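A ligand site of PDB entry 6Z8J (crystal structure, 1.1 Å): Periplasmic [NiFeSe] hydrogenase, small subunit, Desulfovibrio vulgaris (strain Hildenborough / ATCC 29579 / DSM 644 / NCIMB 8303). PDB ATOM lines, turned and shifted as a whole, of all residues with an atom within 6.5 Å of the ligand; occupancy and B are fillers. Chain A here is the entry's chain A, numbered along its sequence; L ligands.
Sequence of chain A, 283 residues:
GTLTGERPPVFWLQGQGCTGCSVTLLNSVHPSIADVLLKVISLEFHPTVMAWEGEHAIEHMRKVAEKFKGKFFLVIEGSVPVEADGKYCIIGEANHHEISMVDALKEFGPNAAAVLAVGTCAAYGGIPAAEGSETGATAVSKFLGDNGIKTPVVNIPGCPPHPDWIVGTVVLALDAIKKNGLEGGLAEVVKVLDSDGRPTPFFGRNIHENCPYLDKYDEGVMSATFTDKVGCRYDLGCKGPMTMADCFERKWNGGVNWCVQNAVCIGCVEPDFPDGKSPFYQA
ND1 of His 208 binds FE2 of the ligand, 2.1 Å away. SG of Cys 211 is bound to FE4 of the ligand. An iron atom (FE3) of the ligand is bound by the side-chain sulfur (SG) of Cys 232 (2.3 Å). The side-chain sulfur (SG) of Cys 238 binds an iron atom (FE1) of the ligand (2.3 Å). N of Arg 233 sits close to S2 of the ligand. The backbone NH (N) of Leu 214 lies close to a sulfur (S1) of the ligand, at 3.6 Å.
A sulfur (S1) of the ligand sits close to the backbone carbonyl oxygen (O) of Tyr 213 (3.7 Å). Tyr 217 touches the ligand (CB to S1, 3.8 Å). Tyr 234 touches the ligand (CB to S4, 3.7 Å). Gly 240 touches the ligand (CA to S3, 3.7 Å). Pro 241 touches the ligand (CD to S4, 3.8 Å). CG1 of Val 260 touches S2 of the ligand (3.5 Å). Hydrophobic or aromatic side chains within 4 Å of the ligand: His 208, Tyr 217, Tyr 234, Pro 241 and Val 260. 12 residues have an atom within 4 Å of the ligand: His 208, Cys 211, Tyr 213, Leu 214, Tyr 217, Cys 232, Arg 233, Tyr 234, Cys 238, Gly 240, Pro 241 and Val 260. Along chain A the residues within 4 Å of the ligand span positions 208 to 260.
The backbone NH (N) of His 208 is in hydrogen-bond range of the backbone carbonyl oxygen (O) of Gly 240. SG of Cys 211 sits close to N of Tyr 213, 3.4 Å away. N of Tyr 234 sits close to SG of Cys 232. SG of Cys 232 lies close to SD of Met 222, 3.6 Å away. The backbone NH of Cys 238 sits at hydrogen-bond distance from the backbone carbonyl oxygen of Arg 233 (3.2 Å). The side-chain sulfur (SG) of Cys 238 sits close to the backbone NH (N) of Gly 240, at 3.4 Å. O of Val 260 lies within hydrogen-bond range of NE of Arg 233 (2.9 Å). The backbone carbonyl oxygen (O) of Gly 231 lies within hydrogen-bond range of the guanidinium group (NH1) of Arg 233 (2.8 Å).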
ATOM      1  N   ILE A 207      17.490  23.474 -31.214  1.00  0.00           N
ATOM      2  CA  ILE A 207      17.775  23.539 -29.781  1.00  0.00           C
ATOM      3  C   ILE A 207      18.581  22.320 -29.351  1.00  0.00           C
ATOM      4  O   ILE A 207      19.655  22.440 -28.746  1.00  0.00           O
ATOM      5  CB  ILE A 207      16.473  23.654 -28.970  1.00  0.00           C
ATOM      6  CG1 ILE A 207      15.729  24.973 -29.249  1.00  0.00           C
ATOM      7  CG2 ILE A 207      16.759  23.472 -27.477  1.00  0.00           C
ATOM      8  CD1 ILE A 207      16.073  26.131 -28.307  1.00  0.00           C
ATOM      9  N   HIS A 208      18.056  21.134 -29.634  1.00  0.00           N
ATOM     10  CA  HIS A 208      18.628  19.885 -29.136  1.00  0.00           C
ATOM     11  C   HIS A 208      20.066  19.680 -29.604  1.00  0.00           C
ATOM     12  O   HIS A 208      20.937  19.309 -28.822  1.00  0.00           O
ATOM     13  CB  HIS A 208      17.710  18.765 -29.618  1.00  0.00           C
ATOM     14  CG  HIS A 208      18.161  17.373 -29.315  1.00  0.00           C
ATOM     15  ND1 HIS A 208      18.091  16.802 -28.063  1.00  0.00           N
ATOM     16  CD2 HIS A 208      18.624  16.398 -30.139  1.00  0.00           C
ATOM     17  CE1 HIS A 208      18.517  15.559 -28.122  1.00  0.00           C
ATOM     18  NE2 HIS A 208      18.858  15.302 -29.367  1.00  0.00           N
ATOM     19  N   GLU A 209      20.326  19.932 -30.883  1.00  0.00           N
ATOM     20  CA  GLU A 209      21.693  19.754 -31.393  1.00  0.00           C
ATOM     21  C   GLU A 209      22.695  20.649 -30.665  1.00  0.00           C
ATOM     22  O   GLU A 209      23.896  20.349 -30.675  1.00  0.00           O
ATOM     23  CB  GLU A 209      21.714  20.076 -32.881  1.00  0.00           C
ATOM     24  CG  GLU A 209      20.959  19.070 -33.742  1.00  0.00           C
ATOM     25  CD  GLU A 209      20.774  19.535 -35.178  1.00  0.00           C
ATOM     26  OE1 GLU A 209      19.792  19.096 -35.820  1.00  0.00           O
ATOM     27  OE2 GLU A 209      21.593  20.359 -35.649  1.00  0.00           O
ATOM     28  N   CYS A 211      22.172  21.744 -27.336  1.00  0.00           N
ATOM     29  CA  CYS A 211      21.750  21.807 -25.953  1.00  0.00           C
ATOM     30  C   CYS A 211      22.880  21.372 -25.016  1.00  0.00           C
ATOM     31  O   CYS A 211      23.593  20.417 -25.316  1.00  0.00           O
ATOM     32  CB  CYS A 211      20.548  20.879 -25.739  1.00  0.00           C
ATOM     33  SG  CYS A 211      19.954  20.849 -24.038  1.00  0.00           S
ATOM     34  N   PRO A 212      23.046  22.051 -23.878  1.00  0.00           N
ATOM     35  CA  PRO A 212      24.078  21.620 -22.915  1.00  0.00           C
ATOM     36  C   PRO A 212      23.864  20.228 -22.324  1.00  0.00           C
ATOM     37  O   PRO A 212      24.833  19.658 -21.797  1.00  0.00           O
ATOM     38  CB  PRO A 212      24.047  22.721 -21.849  1.00  0.00           C
ATOM     39  CG  PRO A 212      22.706  23.338 -21.968  1.00  0.00           C
ATOM     40  CD  PRO A 212      22.337  23.256 -23.422  1.00  0.00           C
ATOM     41  N   TYR A 213      22.670  19.668 -22.402  1.00  0.00           N
ATOM     42  CA  TYR A 213      22.380  18.334 -21.871  1.00  0.00           C
ATOM     43  C   TYR A 213      22.432  17.238 -22.926  1.00  0.00           C
ATOM     44  O   TYR A 213      22.051  16.095 -22.654  1.00  0.00           O
ATOM     45  CB  TYR A 213      21.022  18.339 -21.143  1.00  0.00           C
ATOM     46  CG  TYR A 213      20.943  19.485 -20.195  1.00  0.00           C
ATOM     47  CD1 TYR A 213      21.758  19.541 -19.072  1.00  0.00           C
ATOM     48  CD2 TYR A 213      20.087  20.542 -20.434  1.00  0.00           C
ATOM     49  CE1 TYR A 213      21.723  20.616 -18.221  1.00  0.00           C
ATOM     50  CE2 TYR A 213      20.030  21.623 -19.587  1.00  0.00           C
ATOM     51  CZ  TYR A 213      20.854  21.658 -18.483  1.00  0.00           C
ATOM     52  OH  TYR A 213      20.766  22.749 -17.664  1.00  0.00           O
ATOM     53  N   LEU A 214      22.894  17.571 -24.144  1.00  0.00           N
ATOM     54  CA  LEU A 214      22.908  16.594 -25.225  1.00  0.00           C
ATOM     55  C   LEU A 214      23.738  15.370 -24.869  1.00  0.00           C
ATOM     56  O   LEU A 214      23.377  14.246 -25.241  1.00  0.00           O
ATOM     57  CB  LEU A 214      23.402  17.249 -26.514  1.00  0.00           C
ATOM     58  CG  LEU A 214      23.365  16.367 -27.780  1.00  0.00           C
ATOM     59  CD1 LEU A 214      21.959  15.877 -28.120  1.00  0.00           C
ATOM     60  CD2 LEU A 214      23.945  17.122 -28.957  1.00  0.00           C
ATOM     61  N   ASP A 215      24.847  15.563 -24.146  1.00  0.00           N
ATOM     62  CA  ASP A 215      25.649  14.423 -23.698  1.00  0.00           C
ATOM     63  C   ASP A 215      24.811  13.469 -22.852  1.00  0.00           C
ATOM     64  O   ASP A 215      24.890  12.242 -23.014  1.00  0.00           O
ATOM     65  CB  ASP A 215      26.852  14.924 -22.891  1.00  0.00           C
ATOM     66  CG  ASP A 215      28.170  14.326 -23.366  1.00  0.00           C
ATOM     67  OD1 ASP A 215      28.227  13.094 -23.603  1.00  0.00           O
ATOM     68  OD2 ASP A 215      29.157  15.098 -23.497  1.00  0.00           O
ATOM     69  N   LYS A 216      23.982  14.013 -21.953  1.00  0.00           N
ATOM     70  CA  LYS A 216      23.127  13.160 -21.121  1.00  0.00           C
ATOM     71  C   LYS A 216      22.074  12.437 -21.965  1.00  0.00           C
ATOM     72  O   LYS A 216      21.788  11.261 -21.726  1.00  0.00           O
ATOM     73  CB  LYS A 216      22.448  14.007 -20.050  1.00  0.00           C
ATOM     74  CG  LYS A 216      23.431  14.738 -19.146  1.00  0.00           C
ATOM     75  CD  LYS A 216      24.293  13.769 -18.357  1.00  0.00           C
ATOM     76  CE  LYS A 216      25.063  14.492 -17.267  1.00  0.00           C
ATOM     77  NZ  LYS A 216      26.304  13.794 -16.940  1.00  0.00           N
ATOM     78  N   TYR A 217      21.485  13.125 -22.941  1.00  0.00           N
ATOM     79  CA  TYR A 217      20.564  12.467 -23.858  1.00  0.00           C
ATOM     80  C   TYR A 217      21.238  11.275 -24.522  1.00  0.00           C
ATOM     81  O   TYR A 217      20.713  10.164 -24.528  1.00  0.00           O
ATOM     82  CB  TYR A 217      20.086  13.462 -24.913  1.00  0.00           C
ATOM     83  CG  TYR A 217      19.202  12.885 -25.977  1.00  0.00           C
ATOM     84  CD1 TYR A 217      17.817  12.893 -25.844  1.00  0.00           C
ATOM     85  CD2 TYR A 217      19.735  12.368 -27.144  1.00  0.00           C
ATOM     86  CE1 TYR A 217      16.998  12.381 -26.828  1.00  0.00           C
ATOM     87  CE2 TYR A 217      18.918  11.856 -28.142  1.00  0.00           C
ATOM     88  CZ  TYR A 217      17.558  11.863 -27.983  1.00  0.00           C
ATOM     89  OH  TYR A 217      16.753  11.346 -28.986  1.00  0.00           O
ATOM     90  N   ASP A 218      22.437  11.498 -25.070  1.00  0.00           N
ATOM     91  CA  ASP A 218      23.160  10.430 -25.759  1.00  0.00           C
ATOM     92  C   ASP A 218      23.486   9.270 -24.818  1.00  0.00           C
ATOM     93  O   ASP A 218      23.561   8.119 -25.257  1.00  0.00           O
ATOM     94  CB  ASP A 218      24.426  11.001 -26.387  1.00  0.00           C
ATOM     95  CG  ASP A 218      24.160  11.806 -27.649  1.00  0.00           C
ATOM     96  OD1 ASP A 218      23.052  11.731 -28.211  1.00  0.00           O
ATOM     97  OD2 ASP A 218      25.086  12.526 -28.090  1.00  0.00           O
ATOM     98  N   MET A 222      18.429  10.444 -17.889  1.00  0.00           N
ATOM     99  CA  MET A 222      17.241  11.274 -17.926  1.00  0.00           C
ATOM    100  C   MET A 222      16.794  11.656 -16.517  1.00  0.00           C
ATOM    101  O   MET A 222      16.832  10.830 -15.595  1.00  0.00           O
ATOM    102  CB  MET A 222      16.062  10.524 -18.568  1.00  0.00           C
ATOM    103  CG  MET A 222      16.302  10.094 -19.975  1.00  0.00           C
ATOM    104  SD  MET A 222      16.381  11.518 -21.028  1.00  0.00           S
ATOM    105  CE  MET A 222      17.043  10.801 -22.531  1.00  0.00           C
ATOM    106  N   GLY A 231      20.115  15.441 -15.431  1.00  0.00           N
ATOM    107  CA  GLY A 231      19.791  14.646 -16.592  1.00  0.00           C
ATOM    108  C   GLY A 231      19.130  15.435 -17.706  1.00  0.00           C
ATOM    109  O   GLY A 231      18.675  16.559 -17.533  1.00  0.00           O
ATOM    110  N   CYS A 232      19.053  14.773 -18.850  1.00  0.00           N
ATOM    111  CA  CYS A 232      18.276  15.289 -19.967  1.00  0.00           C
ATOM    112  C   CYS A 232      16.788  15.306 -19.615  1.00  0.00           C
ATOM    113  O   CYS A 232      16.305  14.498 -18.806  1.00  0.00           O
ATOM    114  CB  CYS A 232      18.560  14.400 -21.184  1.00  0.00           C
ATOM    115  SG  CYS A 232      17.461  14.638 -22.575  1.00  0.00           S
ATOM    116  N   ARG A 233      16.071  16.255 -20.213  1.00  0.00           N
ATOM    117  CA  ARG A 233      14.660  16.527 -19.929  1.00  0.00           C
ATOM    118  C   ARG A 233      13.718  15.828 -20.913  1.00  0.00           C
ATOM    119  O   ARG A 233      12.514  16.068 -20.865  1.00  0.00           O
ATOM    120  CB  ARG A 233      14.401  18.030 -19.952  1.00  0.00           C
ATOM    121  CG  ARG A 233      14.971  18.839 -18.792  1.00  0.00           C
ATOM    122  CD  ARG A 233      16.469  18.922 -18.694  1.00  0.00           C
ATOM    123  NE  ARG A 233      16.828  20.114 -17.923  1.00  0.00           N
ATOM    124  CZ  ARG A 233      17.918  20.270 -17.180  1.00  0.00           C
ATOM    125  NH1 ARG A 233      18.827  19.308 -17.079  1.00  0.00           N
ATOM    126  NH2 ARG A 233      18.094  21.413 -16.525  1.00  0.00           N
ATOM    127  N   TYR A 234      14.245  14.973 -21.780  1.00  0.00           N
ATOM    128  CA  TYR A 234      13.420  14.356 -22.826  1.00  0.00           C
ATOM    129  C   TYR A 234      12.232  13.607 -22.250  1.00  0.00           C
ATOM    130  O   TYR A 234      11.098  13.730 -22.738  1.00  0.00           O
ATOM    131  CB  TYR A 234      14.284  13.423 -23.675  1.00  0.00           C
ATOM    132  CG  TYR A 234      13.530  12.738 -24.771  1.00  0.00           C
ATOM    133  CD1 TYR A 234      13.288  13.379 -25.972  1.00  0.00           C
ATOM    134  CD2 TYR A 234      13.054  11.437 -24.610  1.00  0.00           C
ATOM    135  CE1 TYR A 234      12.604  12.750 -26.986  1.00  0.00           C
ATOM    136  CE2 TYR A 234      12.377  10.800 -25.623  1.00  0.00           C
ATOM    137  CZ  TYR A 234      12.161  11.464 -26.813  1.00  0.00           C
ATOM    138  OH  TYR A 234      11.470  10.819 -27.813  1.00  0.00           O
ATOM    139  N   ASP A 235      12.456  12.763 -21.238  1.00  0.00           N
ATOM    140  CA  ASP A 235      11.361  11.964 -20.708  1.00  0.00           C
ATOM    141  C   ASP A 235      10.325  12.815 -19.986  1.00  0.00           C
ATOM    142  O   ASP A 235       9.183  12.375 -19.830  1.00  0.00           O
ATOM    143  CB  ASP A 235      11.895  10.895 -19.742  1.00  0.00           C
ATOM    144  CG  ASP A 235      12.535   9.706 -20.455  1.00  0.00           C
ATOM    145  OD1 ASP A 235      12.528   9.662 -21.704  1.00  0.00           O
ATOM    146  OD2 ASP A 235      13.034   8.794 -19.759  1.00  0.00           O
ATOM    147  N   CYS A 238      10.556  17.322 -23.011  1.00  0.00           N
ATOM    148  CA  CYS A 238      11.269  18.346 -23.767  1.00  0.00           C
ATOM    149  C   CYS A 238      11.122  18.147 -25.271  1.00  0.00           C
ATOM    150  O   CYS A 238      11.390  17.056 -25.801  1.00  0.00           O
ATOM    151  CB  CYS A 238      12.746  18.294 -23.394  1.00  0.00           C
ATOM    152  SG  CYS A 238      13.693  19.642 -24.164  1.00  0.00           S
ATOM    153  N   LYS A 239      10.730  19.209 -25.961  1.00  0.00           N
ATOM    154  CA  LYS A 239      10.574  19.179 -27.409  1.00  0.00           C
ATOM    155  C   LYS A 239      11.742  19.822 -28.143  1.00  0.00           C
ATOM    156  O   LYS A 239      11.628  20.102 -29.337  1.00  0.00           O
ATOM    157  CB  LYS A 239       9.260  19.858 -27.813  1.00  0.00           C
ATOM    158  CG  LYS A 239       8.016  19.220 -27.157  1.00  0.00           C
ATOM    159  CD  LYS A 239       7.957  17.702 -27.325  1.00  0.00           C
ATOM    160  CE  LYS A 239       6.601  17.140 -26.899  1.00  0.00           C
ATOM    161  NZ  LYS A 239       6.285  17.508 -25.503  1.00  0.00           N
ATOM    162  N   GLY A 240      12.865  20.059 -27.455  1.00  0.00           N
ATOM    163  CA  GLY A 240      14.050  20.546 -28.115  1.00  0.00           C
ATOM    164  C   GLY A 240      14.421  19.830 -29.396  1.00  0.00           C
ATOM    165  O   GLY A 240      14.853  20.493 -30.358  1.00  0.00           O
ATOM    166  N   PRO A 241      14.284  18.513 -29.463  1.00  0.00           N
ATOM    167  CA  PRO A 241      14.680  17.802 -30.681  1.00  0.00           C
ATOM    168  C   PRO A 241      13.976  18.287 -31.935  1.00  0.00           C
ATOM    169  O   PRO A 241      14.546  18.173 -33.031  1.00  0.00           O
ATOM    170  CB  PRO A 241      14.358  16.329 -30.358  1.00  0.00           C
ATOM    171  CG  PRO A 241      14.540  16.243 -28.880  1.00  0.00           C
ATOM    172  CD  PRO A 241      13.995  17.563 -28.364  1.00  0.00           C
ATOM    173  N   TRP A 258      16.438  29.818 -19.041  1.00  0.00           N
ATOM    174  CA  TRP A 258      15.719  29.448 -20.257  1.00  0.00           C
ATOM    175  C   TRP A 258      14.917  28.196 -19.961  1.00  0.00           C
ATOM    176  O   TRP A 258      15.097  27.539 -18.935  1.00  0.00           O
ATOM    177  CB  TRP A 258      16.634  29.292 -21.464  1.00  0.00           C
ATOM    178  CG  TRP A 258      17.586  28.144 -21.443  1.00  0.00           C
ATOM    179  CD1 TRP A 258      18.573  27.901 -20.530  1.00  0.00           C
ATOM    180  CD2 TRP A 258      17.688  27.112 -22.434  1.00  0.00           C
ATOM    181  NE1 TRP A 258      19.282  26.779 -20.882  1.00  0.00           N
ATOM    182  CE2 TRP A 258      18.763  26.267 -22.044  1.00  0.00           C
ATOM    183  CE3 TRP A 258      16.995  26.818 -23.620  1.00  0.00           C
ATOM    184  CZ2 TRP A 258      19.166  25.165 -22.808  1.00  0.00           C
ATOM    185  CZ3 TRP A 258      17.377  25.692 -24.359  1.00  0.00           C
ATOM    186  CH2 TRP A 258      18.453  24.889 -23.955  1.00  0.00           C
ATOM    187  N   VAL A 260      14.676  25.077 -21.019  1.00  0.00           N
ATOM    188  CA  VAL A 260      15.231  23.752 -20.801  1.00  0.00           C
ATOM    189  C   VAL A 260      15.940  23.673 -19.461  1.00  0.00           C
ATOM    190  O   VAL A 260      15.858  22.662 -18.762  1.00  0.00           O
ATOM    191  CB  VAL A 260      16.133  23.335 -21.972  1.00  0.00           C
ATOM    192  CG1 VAL A 260      16.887  22.025 -21.691  1.00  0.00           C
ATOM    193  CG2 VAL A 260      15.304  23.237 -23.268  1.00  0.00           C
ATOM    194  N   CYS A 265      11.478  22.502 -22.883  1.00  0.00           N
ATOM    195  CA  CYS A 265      11.033  23.243 -24.072  1.00  0.00           C
ATOM    196  C   CYS A 265       9.695  22.668 -24.541  1.00  0.00           C
ATOM    197  O   CYS A 265       9.525  21.439 -24.617  1.00  0.00           O
ATOM    198  CB  CYS A 265      12.087  23.099 -25.170  1.00  0.00           C
ATOM    199  SG  CYS A 265      11.667  23.862 -26.787  1.00  0.00           S
HETATM  200 FE1  LIG L   1      15.773  18.662 -24.385  1.00  0.00          FE
HETATM  201 FE2  LIG L   1      17.512  17.546 -26.196  1.00  0.00          FE
HETATM  202 FE3  LIG L   1      17.559  16.664 -23.655  1.00  0.00          FE
HETATM  203 FE4  LIG L   1      18.450  19.166 -24.270  1.00  0.00          FE
HETATM  204  S1  LIG L   1      19.382  17.192 -24.910  1.00  0.00           S
HETATM  205  S2  LIG L   1      17.117  18.577 -22.497  1.00  0.00           S
HETATM  206  S3  LIG L   1      16.999  19.767 -25.974  1.00  0.00           S
HETATM  207  S4  LIG L   1      15.774  16.498 -25.135  1.00  0.00           S
